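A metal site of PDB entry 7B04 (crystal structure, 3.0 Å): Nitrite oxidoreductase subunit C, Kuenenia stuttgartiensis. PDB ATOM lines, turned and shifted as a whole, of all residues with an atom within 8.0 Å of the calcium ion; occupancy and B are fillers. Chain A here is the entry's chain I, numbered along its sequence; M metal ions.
Of the 23 residues printed, 6 come within 4 Å of the calcium ion.
The nearest printed residue that does not touch the calcium ion is Gln 250 (4.4 Å).
OD2 of Asp 235 is bound to the calcium ion.
OD2 of Asp 251 is bound to the calcium ion (2.3 Å).
O of His 249 is bound to the calcium ion, at 2.3 Å.
The calcium ion is bound by OD1 of Asp 278 (2.4 Å).
NE2 of Gln 247 binds the calcium ion (2.4 Å).
The calcium ion is bound by OD2 of Asp 275.
The calcium ion is bound by OD2 of Asp 278 (2.6 Å).
N of Asp 235 lies within hydrogen-bond range of OE1 of Gln 250.
OD2 of Asp 278 lies close to NH1 of Arg 269 (3.8 Å).
The side-chain amide nitrogen (NE2) of Gln 280 lies within hydrogen-bond range of the backbone carbonyl oxygen (O) of Asp 278, 3.2 Å away.
The side-chain amide oxygen (OE1) of Gln 247 sits close to the backbone carbonyl oxygen (O) of Leu 277 (2.9 Å).
O of Leu 236 sits close to OE1 of Gln 247.
The side-chain amide nitrogen (ND2) of Asn 237 sits at hydrogen-bond distance from the side-chain amide oxygen (OE1) of Gln 247, 2.8 Å away.
OD1 of Asp 275 lies close to N of Leu 277, at 3.3 Å.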
ATOM      1  N   ASN A 163      24.266   6.944  18.787  1.00  0.00           N
ATOM      2  CA  ASN A 163      24.920   7.039  17.492  1.00  0.00           C
ATOM      3  C   ASN A 163      25.395   8.473  17.302  1.00  0.00           C
ATOM      4  O   ASN A 163      24.640   9.415  17.556  1.00  0.00           O
ATOM      5  CB  ASN A 163      23.965   6.637  16.361  1.00  0.00           C
ATOM      6  CG  ASN A 163      24.673   6.339  15.042  1.00  0.00           C
ATOM      7  OD1 ASN A 163      24.080   5.736  14.139  1.00  0.00           O
ATOM      8  ND2 ASN A 163      25.916   6.768  14.908  1.00  0.00           N
ATOM      9  N   LEU A 164      26.635   8.641  16.842  1.00  0.00           N
ATOM     10  CA  LEU A 164      27.228   9.954  16.606  1.00  0.00           C
ATOM     11  C   LEU A 164      27.747  10.025  15.178  1.00  0.00           C
ATOM     12  O   LEU A 164      28.315   9.057  14.658  1.00  0.00           O
ATOM     13  CB  LEU A 164      28.368  10.241  17.582  1.00  0.00           C
ATOM     14  CG  LEU A 164      28.029  10.507  19.054  1.00  0.00           C
ATOM     15  CD1 LEU A 164      27.949   9.196  19.810  1.00  0.00           C
ATOM     16  CD2 LEU A 164      29.064  11.419  19.678  1.00  0.00           C
ATOM     17  N   TRP A 165      27.562  11.181  14.550  1.00  0.00           N
ATOM     18  CA  TRP A 165      28.107  11.466  13.223  1.00  0.00           C
ATOM     19  C   TRP A 165      29.035  12.662  13.341  1.00  0.00           C
ATOM     20  O   TRP A 165      28.563  13.786  13.531  1.00  0.00           O
ATOM     21  CB  TRP A 165      27.000  11.750  12.209  1.00  0.00           C
ATOM     22  CG  TRP A 165      25.967  10.678  12.071  1.00  0.00           C
ATOM     23  CD1 TRP A 165      26.027   9.401  12.551  1.00  0.00           C
ATOM     24  CD2 TRP A 165      24.719  10.795  11.378  1.00  0.00           C
ATOM     25  NE1 TRP A 165      24.881   8.720  12.210  1.00  0.00           N
ATOM     26  CE2 TRP A 165      24.062   9.553  11.490  1.00  0.00           C
ATOM     27  CE3 TRP A 165      24.088  11.819  10.674  1.00  0.00           C
ATOM     28  CZ2 TRP A 165      22.809   9.312  10.936  1.00  0.00           C
ATOM     29  CZ3 TRP A 165      22.845  11.585  10.128  1.00  0.00           C
ATOM     30  CH2 TRP A 165      22.219  10.338  10.255  1.00  0.00           C
ATOM     31  N   ARG A 231      36.183   9.500   3.013  1.00  0.00           N
ATOM     32  CA  ARG A 231      34.986   9.971   3.690  1.00  0.00           C
ATOM     33  C   ARG A 231      35.255  11.275   4.411  1.00  0.00           C
ATOM     34  O   ARG A 231      36.405  11.626   4.707  1.00  0.00           O
ATOM     35  CB  ARG A 231      34.487   8.940   4.685  1.00  0.00           C
ATOM     36  CG  ARG A 231      33.365   8.091   4.183  1.00  0.00           C
ATOM     37  CD  ARG A 231      32.494   7.678   5.345  1.00  0.00           C
ATOM     38  NE  ARG A 231      32.641   6.263   5.613  1.00  0.00           N
ATOM     39  CZ  ARG A 231      31.779   5.343   5.191  1.00  0.00           C
ATOM     40  NH1 ARG A 231      31.988   4.065   5.472  1.00  0.00           N
ATOM     41  NH2 ARG A 231      30.737   5.692   4.452  1.00  0.00           N
ATOM     42  N   ASP A 235      31.270   7.501  11.483  1.00  0.00           N
ATOM     43  CA  ASP A 235      30.131   6.798  12.133  1.00  0.00           C
ATOM     44  C   ASP A 235      30.627   6.403  13.510  1.00  0.00           C
ATOM     45  O   ASP A 235      31.527   5.615  13.560  1.00  0.00           O
ATOM     46  CB  ASP A 235      29.779   5.514  11.363  1.00  0.00           C
ATOM     47  CG  ASP A 235      28.404   4.921  11.629  1.00  0.00           C
ATOM     48  OD1 ASP A 235      27.514   5.697  11.850  1.00  0.00           O
ATOM     49  OD2 ASP A 235      28.246   3.697  11.575  1.00  0.00           O
ATOM     50  N   LEU A 236      29.992   6.859  14.576  1.00  0.00           N
ATOM     51  CA  LEU A 236      30.513   6.555  15.921  1.00  0.00           C
ATOM     52  C   LEU A 236      29.400   6.147  16.875  1.00  0.00           C
ATOM     53  O   LEU A 236      28.276   6.474  16.658  1.00  0.00           O
ATOM     54  CB  LEU A 236      31.150   7.818  16.486  1.00  0.00           C
ATOM     55  CG  LEU A 236      32.439   8.250  15.831  1.00  0.00           C
ATOM     56  CD1 LEU A 236      32.459   9.750  15.677  1.00  0.00           C
ATOM     57  CD2 LEU A 236      33.592   7.809  16.698  1.00  0.00           C
ATOM     58  N   ASN A 237      29.809   5.480  17.937  1.00  0.00           N
ATOM     59  CA  ASN A 237      28.956   5.061  19.034  1.00  0.00           C
ATOM     60  C   ASN A 237      29.500   5.619  20.341  1.00  0.00           C
ATOM     61  O   ASN A 237      30.690   5.922  20.460  1.00  0.00           O
ATOM     62  CB  ASN A 237      28.889   3.532  19.141  1.00  0.00           C
ATOM     63  CG  ASN A 237      27.664   2.949  18.488  1.00  0.00           C
ATOM     64  OD1 ASN A 237      27.571   1.749  18.270  1.00  0.00           O
ATOM     65  ND2 ASN A 237      26.702   3.811  18.178  1.00  0.00           N
ATOM     66  N   SER A 246      34.612   4.362  17.644  1.00  0.00           N
ATOM     67  CA  SER A 246      34.370   4.411  16.211  1.00  0.00           C
ATOM     68  C   SER A 246      33.777   3.078  15.785  1.00  0.00           C
ATOM     69  O   SER A 246      34.295   2.015  16.136  1.00  0.00           O
ATOM     70  CB  SER A 246      35.658   4.688  15.450  1.00  0.00           C
ATOM     71  OG  SER A 246      35.377   5.215  14.157  1.00  0.00           O
ATOM     72  N   GLN A 247      32.685   3.127  15.028  1.00  0.00           N
ATOM     73  CA  GLN A 247      32.056   1.888  14.603  1.00  0.00           C
ATOM     74  C   GLN A 247      32.892   1.264  13.493  1.00  0.00           C
ATOM     75  O   GLN A 247      33.548   1.961  12.711  1.00  0.00           O
ATOM     76  CB  GLN A 247      30.622   2.147  14.144  1.00  0.00           C
ATOM     77  CG  GLN A 247      29.682   2.582  15.281  1.00  0.00           C
ATOM     78  CD  GLN A 247      28.249   2.751  14.827  1.00  0.00           C
ATOM     79  OE1 GLN A 247      27.401   3.276  15.552  1.00  0.00           O
ATOM     80  NE2 GLN A 247      27.958   2.301  13.611  1.00  0.00           N
ATOM     81  N   ASP A 248      32.837  -0.067  13.405  1.00  0.00           N
ATOM     82  CA  ASP A 248      33.606  -0.756  12.384  1.00  0.00           C
ATOM     83  C   ASP A 248      33.017  -0.524  11.004  1.00  0.00           C
ATOM     84  O   ASP A 248      33.754  -0.329  10.026  1.00  0.00           O
ATOM     85  CB  ASP A 248      33.642  -2.262  12.672  1.00  0.00           C
ATOM     86  CG  ASP A 248      34.392  -2.596  13.951  1.00  0.00           C
ATOM     87  OD1 ASP A 248      35.216  -1.775  14.389  1.00  0.00           O
ATOM     88  OD2 ASP A 248      34.135  -3.686  14.509  1.00  0.00           O
ATOM     89  N   HIS A 249      31.700  -0.497  10.905  1.00  0.00           N
ATOM     90  CA  HIS A 249      31.002  -0.327   9.634  1.00  0.00           C
ATOM     91  C   HIS A 249      30.486   1.109   9.599  1.00  0.00           C
ATOM     92  O   HIS A 249      29.480   1.430  10.230  1.00  0.00           O
ATOM     93  CB  HIS A 249      29.871  -1.338   9.506  1.00  0.00           C
ATOM     94  CG  HIS A 249      29.355  -1.500   8.120  1.00  0.00           C
ATOM     95  ND1 HIS A 249      28.786  -0.464   7.412  1.00  0.00           N
ATOM     96  CD2 HIS A 249      29.303  -2.581   7.300  1.00  0.00           C
ATOM     97  CE1 HIS A 249      28.422  -0.896   6.218  1.00  0.00           C
ATOM     98  NE2 HIS A 249      28.728  -2.181   6.126  1.00  0.00           N
ATOM     99  N   GLN A 250      31.172   1.950   8.847  1.00  0.00           N
ATOM    100  CA  GLN A 250      30.818   3.357   8.762  1.00  0.00           C
ATOM    101  C   GLN A 250      29.847   3.557   7.597  1.00  0.00           C
ATOM    102  O   GLN A 250      30.117   3.095   6.478  1.00  0.00           O
ATOM    103  CB  GLN A 250      32.057   4.224   8.590  1.00  0.00           C
ATOM    104  CG  GLN A 250      33.231   3.748   9.427  1.00  0.00           C
ATOM    105  CD  GLN A 250      33.292   4.447  10.763  1.00  0.00           C
ATOM    106  OE1 GLN A 250      32.533   5.375  11.021  1.00  0.00           O
ATOM    107  NE2 GLN A 250      34.177   3.989  11.640  1.00  0.00           N
ATOM    108  N   ASP A 251      28.737   4.241   7.862  1.00  0.00           N
ATOM    109  CA  ASP A 251      27.663   4.377   6.899  1.00  0.00           C
ATOM    110  C   ASP A 251      27.328   5.810   6.544  1.00  0.00           C
ATOM    111  O   ASP A 251      26.620   6.038   5.556  1.00  0.00           O
ATOM    112  CB  ASP A 251      26.368   3.718   7.419  1.00  0.00           C
ATOM    113  CG  ASP A 251      26.611   2.355   8.041  1.00  0.00           C
ATOM    114  OD1 ASP A 251      26.897   1.392   7.301  1.00  0.00           O
ATOM    115  OD2 ASP A 251      26.517   2.249   9.278  1.00  0.00           O
ATOM    116  N   VAL A 252      27.824   6.783   7.297  1.00  0.00           N
ATOM    117  CA  VAL A 252      27.496   8.186   7.103  1.00  0.00           C
ATOM    118  C   VAL A 252      28.569   8.840   6.237  1.00  0.00           C
ATOM    119  O   VAL A 252      29.762   8.533   6.373  1.00  0.00           O
ATOM    120  CB  VAL A 252      27.376   8.925   8.450  1.00  0.00           C
ATOM    121  CG1 VAL A 252      28.610   8.706   9.269  1.00  0.00           C
ATOM    122  CG2 VAL A 252      27.164  10.410   8.236  1.00  0.00           C
ATOM    123  N   ARG A 269      23.046  10.133   4.826  1.00  0.00           N
ATOM    124  CA  ARG A 269      23.092   8.710   5.096  1.00  0.00           C
ATOM    125  C   ARG A 269      21.718   8.114   4.801  1.00  0.00           C
ATOM    126  O   ARG A 269      20.704   8.805   4.898  1.00  0.00           O
ATOM    127  CB  ARG A 269      23.496   8.452   6.552  1.00  0.00           C
ATOM    128  CG  ARG A 269      23.766   7.007   6.903  1.00  0.00           C
ATOM    129  CD  ARG A 269      23.408   6.728   8.354  1.00  0.00           C
ATOM    130  NE  ARG A 269      21.983   6.429   8.494  1.00  0.00           N
ATOM    131  CZ  ARG A 269      21.473   5.674   9.462  1.00  0.00           C
ATOM    132  NH1 ARG A 269      22.256   5.153  10.393  1.00  0.00           N
ATOM    133  NH2 ARG A 269      20.165   5.454   9.509  1.00  0.00           N
ATOM    134  N   THR A 273      20.059   1.066   7.714  1.00  0.00           N
ATOM    135  CA  THR A 273      21.336   0.414   7.437  1.00  0.00           C
ATOM    136  C   THR A 273      21.309  -0.981   8.041  1.00  0.00           C
ATOM    137  O   THR A 273      20.610  -1.246   9.024  1.00  0.00           O
ATOM    138  CB  THR A 273      22.522   1.189   8.022  1.00  0.00           C
ATOM    139  OG1 THR A 273      22.348   1.368   9.432  1.00  0.00           O
ATOM    140  CG2 THR A 273      22.659   2.559   7.357  1.00  0.00           C
ATOM    141  N   GLY A 274      22.095  -1.872   7.448  1.00  0.00           N
ATOM    142  CA  GLY A 274      22.217  -3.215   7.979  1.00  0.00           C
ATOM    143  C   GLY A 274      23.032  -3.321   9.244  1.00  0.00           C
ATOM    144  O   GLY A 274      23.114  -4.421   9.822  1.00  0.00           O
ATOM    145  N   ASP A 275      23.627  -2.223   9.703  1.00  0.00           N
ATOM    146  CA  ASP A 275      24.401  -2.230  10.927  1.00  0.00           C
ATOM    147  C   ASP A 275      23.470  -1.992  12.108  1.00  0.00           C
ATOM    148  O   ASP A 275      22.829  -0.934  12.170  1.00  0.00           O
ATOM    149  CB  ASP A 275      25.479  -1.156  10.878  1.00  0.00           C
ATOM    150  CG  ASP A 275      26.466  -1.258  12.031  1.00  0.00           C
ATOM    151  OD1 ASP A 275      26.299  -2.119  12.912  1.00  0.00           O
ATOM    152  OD2 ASP A 275      27.429  -0.457  12.057  1.00  0.00           O
ATOM    153  N   PRO A 276      23.363  -2.931  13.052  1.00  0.00           N
ATOM    154  CA  PRO A 276      22.439  -2.739  14.178  1.00  0.00           C
ATOM    155  C   PRO A 276      22.819  -1.611  15.115  1.00  0.00           C
ATOM    156  O   PRO A 276      21.943  -1.135  15.856  1.00  0.00           O
ATOM    157  CB  PRO A 276      22.479  -4.102  14.897  1.00  0.00           C
ATOM    158  CG  PRO A 276      23.022  -5.069  13.893  1.00  0.00           C
ATOM    159  CD  PRO A 276      23.970  -4.277  13.040  1.00  0.00           C
ATOM    160  N   LEU A 277      24.073  -1.178  15.134  1.00  0.00           N
ATOM    161  CA  LEU A 277      24.515  -0.122  16.040  1.00  0.00           C
ATOM    162  C   LEU A 277      24.257   1.286  15.517  1.00  0.00           C
ATOM    163  O   LEU A 277      24.742   2.254  16.117  1.00  0.00           O
ATOM    164  CB  LEU A 277      26.007  -0.292  16.346  1.00  0.00           C
ATOM    165  CG  LEU A 277      26.360  -1.451  17.281  1.00  0.00           C
ATOM    166  CD1 LEU A 277      27.868  -1.540  17.474  1.00  0.00           C
ATOM    167  CD2 LEU A 277      25.648  -1.313  18.619  1.00  0.00           C
ATOM    168  N   ASP A 278      23.513   1.430  14.427  1.00  0.00           N
ATOM    169  CA  ASP A 278      23.158   2.751  13.900  1.00  0.00           C
ATOM    170  C   ASP A 278      21.703   3.059  14.195  1.00  0.00           C
ATOM    171  O   ASP A 278      20.851   2.174  14.233  1.00  0.00           O
ATOM    172  CB  ASP A 278      23.428   2.832  12.401  1.00  0.00           C
ATOM    173  CG  ASP A 278      24.885   2.636  12.073  1.00  0.00           C
ATOM    174  OD1 ASP A 278      25.439   1.582  12.446  1.00  0.00           O
ATOM    175  OD2 ASP A 278      25.496   3.535  11.441  1.00  0.00           O
ATOM    176  N   VAL A 279      21.413   4.350  14.419  1.00  0.00           N
ATOM    177  CA  VAL A 279      20.031   4.781  14.592  1.00  0.00           C
ATOM    178  C   VAL A 279      19.251   4.497  13.318  1.00  0.00           C
ATOM    179  O   VAL A 279      19.760   4.662  12.198  1.00  0.00           O
ATOM    180  CB  VAL A 279      19.948   6.263  15.006  1.00  0.00           C
ATOM    181  CG1 VAL A 279      20.014   7.197  13.811  1.00  0.00           C
ATOM    182  CG2 VAL A 279      18.666   6.501  15.775  1.00  0.00           C
ATOM    183  N   GLN A 280      18.029   4.024  13.487  1.00  0.00           N
ATOM    184  CA  GLN A 280      17.150   3.653  12.386  1.00  0.00           C
ATOM    185  C   GLN A 280      16.004   4.648  12.301  1.00  0.00           C
ATOM    186  O   GLN A 280      15.240   4.813  13.261  1.00  0.00           O
ATOM    187  CB  GLN A 280      16.625   2.226  12.576  1.00  0.00           C
ATOM    188  CG  GLN A 280      17.707   1.175  12.664  1.00  0.00           C
ATOM    189  CD  GLN A 280      18.525   1.075  11.389  1.00  0.00           C
ATOM    190  OE1 GLN A 280      17.992   1.184  10.280  1.00  0.00           O
ATOM    191  NE2 GLN A 280      19.824   0.859  11.527  1.00  0.00           N
HETATM  192 CA    CA M   1      27.494   1.860  11.339  1.00  0.00          CA
